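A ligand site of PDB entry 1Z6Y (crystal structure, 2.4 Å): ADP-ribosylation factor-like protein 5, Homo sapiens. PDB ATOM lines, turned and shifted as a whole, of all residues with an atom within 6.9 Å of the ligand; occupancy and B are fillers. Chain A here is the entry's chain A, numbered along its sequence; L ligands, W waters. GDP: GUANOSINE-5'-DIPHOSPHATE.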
ATOM      1  N   GLY A  23     -11.183 -30.857  16.239  1.00  0.00           N
ATOM      2  CA  GLY A  23     -10.887 -29.635  16.991  1.00  0.00           C
ATOM      3  C   GLY A  23     -11.542 -29.806  18.349  1.00  0.00           C
ATOM      4  O   GLY A  23     -12.223 -30.801  18.548  1.00  0.00           O
ATOM      5  N   LEU A  24     -11.327 -28.858  19.263  1.00  0.00           N
ATOM      6  CA  LEU A  24     -11.952 -28.874  20.586  1.00  0.00           C
ATOM      7  C   LEU A  24     -13.385 -28.512  20.414  1.00  0.00           C
ATOM      8  O   LEU A  24     -13.798 -27.896  19.389  1.00  0.00           O
ATOM      9  CB  LEU A  24     -11.234 -27.922  21.581  1.00  0.00           C
ATOM     10  CG  LEU A  24      -9.730 -27.987  21.813  1.00  0.00           C
ATOM     11  CD1 LEU A  24      -9.089 -26.642  22.202  1.00  0.00           C
ATOM     12  CD2 LEU A  24      -9.457 -29.051  22.830  1.00  0.00           C
ATOM     13  N   ASP A  25     -14.158 -28.891  21.415  1.00  0.00           N
ATOM     14  CA  ASP A  25     -15.563 -28.534  21.464  1.00  0.00           C
ATOM     15  C   ASP A  25     -15.685 -27.025  21.331  1.00  0.00           C
ATOM     16  O   ASP A  25     -14.862 -26.285  21.875  1.00  0.00           O
ATOM     17  CB  ASP A  25     -16.207 -29.045  22.759  1.00  0.00           C
ATOM     18  CG  ASP A  25     -15.495 -28.552  24.030  1.00  0.00           C
ATOM     19  OD1 ASP A  25     -14.452 -29.128  24.421  1.00  0.00           O
ATOM     20  OD2 ASP A  25     -16.031 -27.593  24.670  1.00  0.00           O
ATOM     21  N   ASN A  26     -16.687 -26.563  20.580  1.00  0.00           N
ATOM     22  CA  ASN A  26     -16.884 -25.122  20.385  1.00  0.00           C
ATOM     23  C   ASN A  26     -15.846 -24.397  19.500  1.00  0.00           C
ATOM     24  O   ASN A  26     -15.860 -23.183  19.404  1.00  0.00           O
ATOM     25  CB  ASN A  26     -17.059 -24.375  21.735  1.00  0.00           C
ATOM     26  CG  ASN A  26     -17.860 -23.086  21.587  1.00  0.00           C
ATOM     27  OD1 ASN A  26     -17.308 -22.034  21.247  1.00  0.00           O
ATOM     28  ND2 ASN A  26     -19.190 -23.160  21.833  1.00  0.00           N
ATOM     29  N   ALA A  27     -14.984 -25.165  18.812  1.00  0.00           N
ATOM     30  CA  ALA A  27     -14.055 -24.600  17.780  1.00  0.00           C
ATOM     31  C   ALA A  27     -14.766 -23.947  16.615  1.00  0.00           C
ATOM     32  O   ALA A  27     -14.323 -22.911  16.108  1.00  0.00           O
ATOM     33  CB  ALA A  27     -13.124 -25.709  17.261  1.00  0.00           C
ATOM     34  N   GLY A  28     -15.871 -24.553  16.173  1.00  0.00           N
ATOM     35  CA  GLY A  28     -16.666 -24.063  15.036  1.00  0.00           C
ATOM     36  C   GLY A  28     -16.766 -25.103  13.915  1.00  0.00           C
ATOM     37  O   GLY A  28     -16.988 -24.734  12.745  1.00  0.00           O
ATOM     38  N   LYS A  29     -16.593 -26.393  14.256  1.00  0.00           N
ATOM     39  CA  LYS A  29     -16.615 -27.513  13.307  1.00  0.00           C
ATOM     40  C   LYS A  29     -17.977 -27.753  12.632  1.00  0.00           C
ATOM     41  O   LYS A  29     -18.061 -27.913  11.413  1.00  0.00           O
ATOM     42  CB  LYS A  29     -16.157 -28.819  13.987  1.00  0.00           C
ATOM     43  CG  LYS A  29     -14.804 -28.806  14.671  1.00  0.00           C
ATOM     44  CD  LYS A  29     -14.519 -30.185  15.288  1.00  0.00           C
ATOM     45  CE  LYS A  29     -15.390 -30.446  16.495  1.00  0.00           C
ATOM     46  NZ  LYS A  29     -15.181 -29.475  17.565  1.00  0.00           N
ATOM     47  N   THR A  30     -19.028 -27.837  13.445  1.00  0.00           N
ATOM     48  CA  THR A  30     -20.422 -27.947  13.007  1.00  0.00           C
ATOM     49  C   THR A  30     -20.914 -26.701  12.200  1.00  0.00           C
ATOM     50  O   THR A  30     -21.645 -26.840  11.204  1.00  0.00           O
ATOM     51  CB  THR A  30     -21.304 -28.176  14.255  1.00  0.00           C
ATOM     52  OG1 THR A  30     -20.937 -29.408  14.870  1.00  0.00           O
ATOM     53  CG2 THR A  30     -22.749 -28.251  13.931  1.00  0.00           C
ATOM     54  N   THR A  31     -20.557 -25.501  12.661  1.00  0.00           N
ATOM     55  CA  THR A  31     -20.919 -24.273  11.928  1.00  0.00           C
ATOM     56  C   THR A  31     -20.350 -24.269  10.522  1.00  0.00           C
ATOM     57  O   THR A  31     -21.004 -23.787   9.626  1.00  0.00           O
ATOM     58  CB  THR A  31     -20.488 -22.954  12.657  1.00  0.00           C
ATOM     59  OG1 THR A  31     -20.736 -23.106  14.046  1.00  0.00           O
ATOM     60  CG2 THR A  31     -21.320 -21.738  12.155  1.00  0.00           C
ATOM     61  N   ILE A  32     -19.134 -24.797  10.378  1.00  0.00           N
ATOM     62  CA  ILE A  32     -18.395 -24.957   9.103  1.00  0.00           C
ATOM     63  C   ILE A  32     -19.030 -25.999   8.186  1.00  0.00           C
ATOM     64  O   ILE A  32     -19.142 -25.769   6.987  1.00  0.00           O
ATOM     65  CB  ILE A  32     -16.900 -25.319   9.309  1.00  0.00           C
ATOM     66  CG1 ILE A  32     -16.146 -24.179  10.031  1.00  0.00           C
ATOM     67  CG2 ILE A  32     -16.209 -25.665   7.939  1.00  0.00           C
ATOM     68  CD1 ILE A  32     -14.679 -24.420  10.278  1.00  0.00           C
ATOM     69  N   MET A  64     -16.444 -36.459  11.852  1.00  0.00           N
ATOM     70  CA  MET A  64     -16.059 -35.441  12.807  1.00  0.00           C
ATOM     71  C   MET A  64     -16.196 -35.773  14.278  1.00  0.00           C
ATOM     72  O   MET A  64     -17.010 -36.570  14.669  1.00  0.00           O
ATOM     73  CB  MET A  64     -16.795 -34.147  12.504  1.00  0.00           C
ATOM     74  CG  MET A  64     -18.069 -34.029  13.200  1.00  0.00           C
ATOM     75  SD  MET A  64     -18.106 -32.449  14.059  1.00  0.00           S
ATOM     76  CE  MET A  64     -18.671 -31.409  12.756  1.00  0.00           C
ATOM     77  N   ASP A  66     -14.895 -34.071  18.452  1.00  0.00           N
ATOM     78  CA  ASP A  66     -14.127 -33.228  19.387  1.00  0.00           C
ATOM     79  C   ASP A  66     -12.914 -33.980  19.957  1.00  0.00           C
ATOM     80  O   ASP A  66     -12.962 -35.202  20.198  1.00  0.00           O
ATOM     81  CB  ASP A  66     -15.003 -32.831  20.564  1.00  0.00           C
ATOM     82  CG  ASP A  66     -16.151 -31.981  20.143  1.00  0.00           C
ATOM     83  OD1 ASP A  66     -16.132 -31.443  19.022  1.00  0.00           O
ATOM     84  OD2 ASP A  66     -17.094 -31.853  20.945  1.00  0.00           O
ATOM     85  N   VAL A  90      -9.954 -27.598  13.082  1.00  0.00           N
ATOM     86  CA  VAL A  90     -10.537 -26.276  13.322  1.00  0.00           C
ATOM     87  C   VAL A  90     -10.018 -25.760  14.671  1.00  0.00           C
ATOM     88  O   VAL A  90     -10.080 -26.452  15.701  1.00  0.00           O
ATOM     89  CB  VAL A  90     -12.100 -26.244  13.222  1.00  0.00           C
ATOM     90  CG1 VAL A  90     -12.584 -24.801  13.088  1.00  0.00           C
ATOM     91  CG2 VAL A  90     -12.666 -27.135  12.043  1.00  0.00           C
ATOM     92  N   ASP A  92     -10.140 -22.518  17.417  1.00  0.00           N
ATOM     93  CA  ASP A  92     -10.753 -21.280  17.881  1.00  0.00           C
ATOM     94  C   ASP A  92      -9.626 -20.240  18.160  1.00  0.00           C
ATOM     95  O   ASP A  92      -8.995 -20.284  19.217  1.00  0.00           O
ATOM     96  CB  ASP A  92     -11.627 -21.545  19.120  1.00  0.00           C
ATOM     97  CG  ASP A  92     -12.218 -20.278  19.705  1.00  0.00           C
ATOM     98  OD1 ASP A  92     -11.969 -19.184  19.133  1.00  0.00           O
ATOM     99  OD2 ASP A  92     -12.907 -20.336  20.741  1.00  0.00           O
ATOM    100  N   ALA A 124      -8.081 -21.362  11.018  1.00  0.00           N
ATOM    101  CA  ALA A 124      -8.016 -20.465  12.113  1.00  0.00           C
ATOM    102  C   ALA A 124      -9.375 -19.725  12.133  1.00  0.00           C
ATOM    103  O   ALA A 124      -9.586 -18.692  11.457  1.00  0.00           O
ATOM    104  CB  ALA A 124      -6.841 -19.505  11.948  1.00  0.00           C
ATOM    105  N   ASN A 125     -10.298 -20.249  12.957  1.00  0.00           N
ATOM    106  CA  ASN A 125     -11.660 -19.799  12.995  1.00  0.00           C
ATOM    107  C   ASN A 125     -11.884 -18.768  14.078  1.00  0.00           C
ATOM    108  O   ASN A 125     -11.060 -18.606  14.991  1.00  0.00           O
ATOM    109  CB  ASN A 125     -12.588 -21.032  13.163  1.00  0.00           C
ATOM    110  CG  ASN A 125     -14.070 -20.704  12.962  1.00  0.00           C
ATOM    111  OD1 ASN A 125     -14.415 -19.909  12.086  1.00  0.00           O
ATOM    112  ND2 ASN A 125     -14.929 -21.286  13.792  1.00  0.00           N
ATOM    113  N   LYS A 126     -13.004 -18.014  13.949  1.00  0.00           N
ATOM    114  CA  LYS A 126     -13.389 -16.963  14.870  1.00  0.00           C
ATOM    115  C   LYS A 126     -12.426 -15.792  14.754  1.00  0.00           C
ATOM    116  O   LYS A 126     -12.122 -15.121  15.759  1.00  0.00           O
ATOM    117  CB  LYS A 126     -13.437 -17.459  16.322  1.00  0.00           C
ATOM    118  CG  LYS A 126     -14.254 -18.723  16.473  1.00  0.00           C
ATOM    119  CD  LYS A 126     -14.799 -18.868  17.841  1.00  0.00           C
ATOM    120  CE  LYS A 126     -15.529 -20.253  17.916  1.00  0.00           C
ATOM    121  NZ  LYS A 126     -16.143 -20.445  19.272  1.00  0.00           N
ATOM    122  N   GLN A 127     -11.958 -15.569  13.524  1.00  0.00           N
ATOM    123  CA  GLN A 127     -11.024 -14.456  13.293  1.00  0.00           C
ATOM    124  C   GLN A 127     -11.762 -13.120  13.197  1.00  0.00           C
ATOM    125  O   GLN A 127     -11.166 -12.096  12.925  1.00  0.00           O
ATOM    126  CB  GLN A 127     -10.178 -14.690  12.046  1.00  0.00           C
ATOM    127  CG  GLN A 127      -9.035 -15.721  12.187  1.00  0.00           C
ATOM    128  CD  GLN A 127      -7.771 -15.156  12.787  1.00  0.00           C
ATOM    129  OE1 GLN A 127      -7.438 -13.974  12.606  1.00  0.00           O
ATOM    130  NE2 GLN A 127      -7.045 -15.995  13.516  1.00  0.00           N
ATOM    131  N   ASP A 128     -13.071 -13.129  13.422  1.00  0.00           N
ATOM    132  CA  ASP A 128     -13.856 -11.921  13.413  1.00  0.00           C
ATOM    133  C   ASP A 128     -13.778 -11.303  14.760  1.00  0.00           C
ATOM    134  O   ASP A 128     -14.083 -10.113  14.908  1.00  0.00           O
ATOM    135  CB  ASP A 128     -15.313 -12.233  13.099  1.00  0.00           C
ATOM    136  CG  ASP A 128     -15.943 -13.164  14.103  1.00  0.00           C
ATOM    137  OD1 ASP A 128     -15.579 -14.361  14.100  1.00  0.00           O
ATOM    138  OD2 ASP A 128     -16.815 -12.732  14.886  1.00  0.00           O
ATOM    139  N   VAL A 129     -13.334 -12.103  15.739  1.00  0.00           N
ATOM    140  CA  VAL A 129     -13.229 -11.645  17.110  1.00  0.00           C
ATOM    141  C   VAL A 129     -11.959 -10.875  17.222  1.00  0.00           C
ATOM    142  O   VAL A 129     -10.904 -11.275  16.673  1.00  0.00           O
ATOM    143  CB  VAL A 129     -13.303 -12.803  18.161  1.00  0.00           C
ATOM    144  CG1 VAL A 129     -13.526 -12.282  19.638  1.00  0.00           C
ATOM    145  CG2 VAL A 129     -14.402 -13.838  17.791  1.00  0.00           C
ATOM    146  N   CYS A 157     -10.638 -17.891   8.868  1.00  0.00           N
ATOM    147  CA  CYS A 157     -12.033 -17.948   8.535  1.00  0.00           C
ATOM    148  C   CYS A 157     -12.985 -17.451   9.645  1.00  0.00           C
ATOM    149  O   CYS A 157     -12.575 -17.227  10.764  1.00  0.00           O
ATOM    150  CB  CYS A 157     -12.412 -19.377   8.111  1.00  0.00           C
ATOM    151  SG  CYS A 157     -12.453 -20.572   9.438  1.00  0.00           S
ATOM    152  N   CYS A 158     -14.250 -17.275   9.280  1.00  0.00           N
ATOM    153  CA  CYS A 158     -15.298 -16.936  10.213  1.00  0.00           C
ATOM    154  C   CYS A 158     -16.452 -17.824   9.769  1.00  0.00           C
ATOM    155  O   CYS A 158     -17.049 -17.543   8.732  1.00  0.00           O
ATOM    156  CB  CYS A 158     -15.704 -15.453  10.118  1.00  0.00           C
ATOM    157  SG  CYS A 158     -17.180 -15.018  11.144  1.00  0.00           S
ATOM    158  N   ALA A 159     -16.744 -18.889  10.538  1.00  0.00           N
ATOM    159  CA  ALA A 159     -17.784 -19.850  10.134  1.00  0.00           C
ATOM    160  C   ALA A 159     -19.152 -19.253  10.061  1.00  0.00           C
ATOM    161  O   ALA A 159     -19.960 -19.673   9.241  1.00  0.00           O
ATOM    162  CB  ALA A 159     -17.792 -21.079  11.020  1.00  0.00           C
ATOM    163  N   LEU A 160     -19.412 -18.233  10.881  1.00  0.00           N
ATOM    164  CA  LEU A 160     -20.733 -17.576  10.906  1.00  0.00           C
ATOM    165  C   LEU A 160     -21.140 -17.013   9.525  1.00  0.00           C
ATOM    166  O   LEU A 160     -22.272 -17.235   9.070  1.00  0.00           O
ATOM    167  CB  LEU A 160     -20.791 -16.488  11.956  1.00  0.00           C
ATOM    168  CG  LEU A 160     -21.400 -16.804  13.329  1.00  0.00           C
ATOM    169  CD1 LEU A 160     -21.226 -18.267  13.754  1.00  0.00           C
ATOM    170  CD2 LEU A 160     -20.832 -15.881  14.356  1.00  0.00           C
ATOM    171  N   THR A 161     -20.210 -16.333   8.856  1.00  0.00           N
ATOM    172  CA  THR A 161     -20.414 -15.789   7.532  1.00  0.00           C
ATOM    173  C   THR A 161     -19.842 -16.675   6.410  1.00  0.00           C
ATOM    174  O   THR A 161     -20.219 -16.508   5.243  1.00  0.00           O
ATOM    175  CB  THR A 161     -19.819 -14.364   7.429  1.00  0.00           C
ATOM    176  OG1 THR A 161     -18.401 -14.445   7.568  1.00  0.00           O
ATOM    177  CG2 THR A 161     -20.402 -13.446   8.538  1.00  0.00           C
HETATM  178  PB  GDP L   1     -18.252 -27.295  17.505  1.00  0.00           P
HETATM  179  O1B GDP L   1     -19.007 -28.079  16.457  1.00  0.00           O
HETATM  180  O2B GDP L   1     -18.467 -27.811  18.901  1.00  0.00           O
HETATM  181  O3B GDP L   1     -16.779 -27.416  17.201  1.00  0.00           O
HETATM  182  O3A GDP L   1     -18.542 -25.733  17.428  1.00  0.00           O
HETATM  183  PA  GDP L   1     -19.805 -24.939  16.893  1.00  0.00           P
HETATM  184  O1A GDP L   1     -19.809 -24.946  15.383  1.00  0.00           O
HETATM  185  O2A GDP L   1     -21.083 -25.283  17.591  1.00  0.00           O
HETATM  186  O5' GDP L   1     -19.447 -23.431  17.320  1.00  0.00           O
HETATM  187  C5' GDP L   1     -19.655 -23.117  18.675  1.00  0.00           C
HETATM  188  C4' GDP L   1     -20.171 -21.694  18.822  1.00  0.00           C
HETATM  189  O4' GDP L   1     -19.257 -20.703  18.322  1.00  0.00           O
HETATM  190  C3' GDP L   1     -21.471 -21.531  18.084  1.00  0.00           C
HETATM  191  O3' GDP L   1     -22.233 -20.808  19.041  1.00  0.00           O
HETATM  192  C2' GDP L   1     -21.194 -20.627  16.915  1.00  0.00           C
HETATM  193  O2' GDP L   1     -22.323 -19.739  16.810  1.00  0.00           O
HETATM  194  C1' GDP L   1     -19.878 -19.915  17.315  1.00  0.00           C
HETATM  195  N9  GDP L   1     -18.970 -19.770  16.156  1.00  0.00           N
HETATM  196  C8  GDP L   1     -18.635 -20.666  15.205  1.00  0.00           C
HETATM  197  N7  GDP L   1     -17.795 -20.098  14.283  1.00  0.00           N
HETATM  198  C5  GDP L   1     -17.599 -18.793  14.645  1.00  0.00           C
HETATM  199  C6  GDP L   1     -16.858 -17.600  14.145  1.00  0.00           C
HETATM  200  O6  GDP L   1     -16.135 -17.638  13.094  1.00  0.00           O
HETATM  201  N1  GDP L   1     -16.968 -16.467  14.887  1.00  0.00           N
HETATM  202  C2  GDP L   1     -17.718 -16.378  16.002  1.00  0.00           C
HETATM  203  N2  GDP L   1     -17.866 -15.214  16.688  1.00  0.00           N
HETATM  204  N3  GDP L   1     -18.402 -17.427  16.503  1.00  0.00           N
HETATM  205  C4  GDP L   1     -18.371 -18.612  15.879  1.00  0.00           C
HETATM  206  O   HOH W   1     -18.147 -18.105  19.374  1.00  0.00           O
HETATM  207  O   HOH W   2     -18.842 -29.977  20.470  1.00  0.00           O
HETATM  208  O   HOH W   3     -23.418 -26.065  15.487  1.00  0.00           O
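The side-chain sulfur (SG) of Cys 157 is in hydrogen-bond range of the side-chain amide oxygen (OD1) of Asn 125 (3.4 Å).
The side-chain carboxylate of Asp 128 is in hydrogen-bond range of the side-chain sulfur of Cys 158.
O of Gly 23 is in hydrogen-bond range of NZ of Lys 29 (3.4 Å).
NZ of Lys 126 lies within salt-bridge range of OD2 of Asp 92, at 3.6 Å.
The backbone carbonyl oxygen of Asn 26 is in hydrogen-bond range of the side-chain amino group of Lys 126, 2.8 Å away.
The side-chain amino group (NZ) of Lys 29 lies within hydrogen-bond range of the backbone carbonyl oxygen (O) of Leu 24, at 2.8 Å.
The side-chain amide nitrogen (ND2) of Asn 125 sits at hydrogen-bond distance from the backbone carbonyl oxygen (O) of Ala 27, at 2.9 Å.
The backbone NH (N) of Ala 159 is in hydrogen-bond range of the side-chain amide oxygen (OD1) of Asn 125 (3.0 Å).
Merely in contact with the ligand: Leu 24, Asp 25, Val 129 and Leu 160.
Hydrophobic or aromatic side chains within 4 Å of the ligand: Val 129, Ala 159 and Leu 160.
Of the 25 residues printed, 15 come within 4 Å of the ligand.
An oxygen (O3B) of the ligand is in hydrogen-bond range of the backbone NH (N) of Ala 27 (3.3 Å).
An oxygen (O4') of the ligand lies within hydrogen-bond range of the side-chain amino group (NZ) of Lys 126 (3.3 Å).
The side-chain carboxylate (OD1) of Asp 128 sits at hydrogen-bond distance from a nitrogen (N1) of the ligand.
The backbone NH (N) of Thr 31 sits at hydrogen-bond distance from an oxygen (O1A) of the ligand, 2.9 Å away.
The backbone NH (N) of Lys 29 lies within hydrogen-bond range of an oxygen (O3B) of the ligand (3.1 Å).
NZ of Lys 29 is in salt-bridge range of O3B of the ligand (2.6 Å).
OG1 of Thr 30 lies within hydrogen-bond range of O1B of the ligand (2.8 Å).
O1A of the ligand is in hydrogen-bond range of OG1 of Thr 31, 2.5 Å away.
The backbone NH (N) of Asn 26 sits at hydrogen-bond distance from an oxygen (O2B) of the ligand, at 2.7 Å.
N of Thr 30 lies within hydrogen-bond range of O1B of the ligand, 3.0 Å away.
N of Ala 159 lies within hydrogen-bond range of O6 of the ligand (2.9 Å).
The side-chain sulfur of Cys 158 lies close to an oxygen (O6) of the ligand, 3.4 Å away.
O6 of the ligand sits at hydrogen-bond distance from N of Lys 126 (3.3 Å).
The side-chain amide oxygen (OD1) of Asn 125 sits close to an oxygen (O6) of the ligand.
An oxygen (O3B) of the ligand sits at hydrogen-bond distance from the backbone NH (N) of Gly 28 (3.2 Å).
Water W2 lies within hydrogen-bond range of the side-chain carboxylate of Asp 66 (2.6 Å) and an oxygen (O2B) of the ligand (2.7 Å).
Water W1 bridges N3 of the ligand (3.0 Å) and NZ of Lys 126 (3.1 Å).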
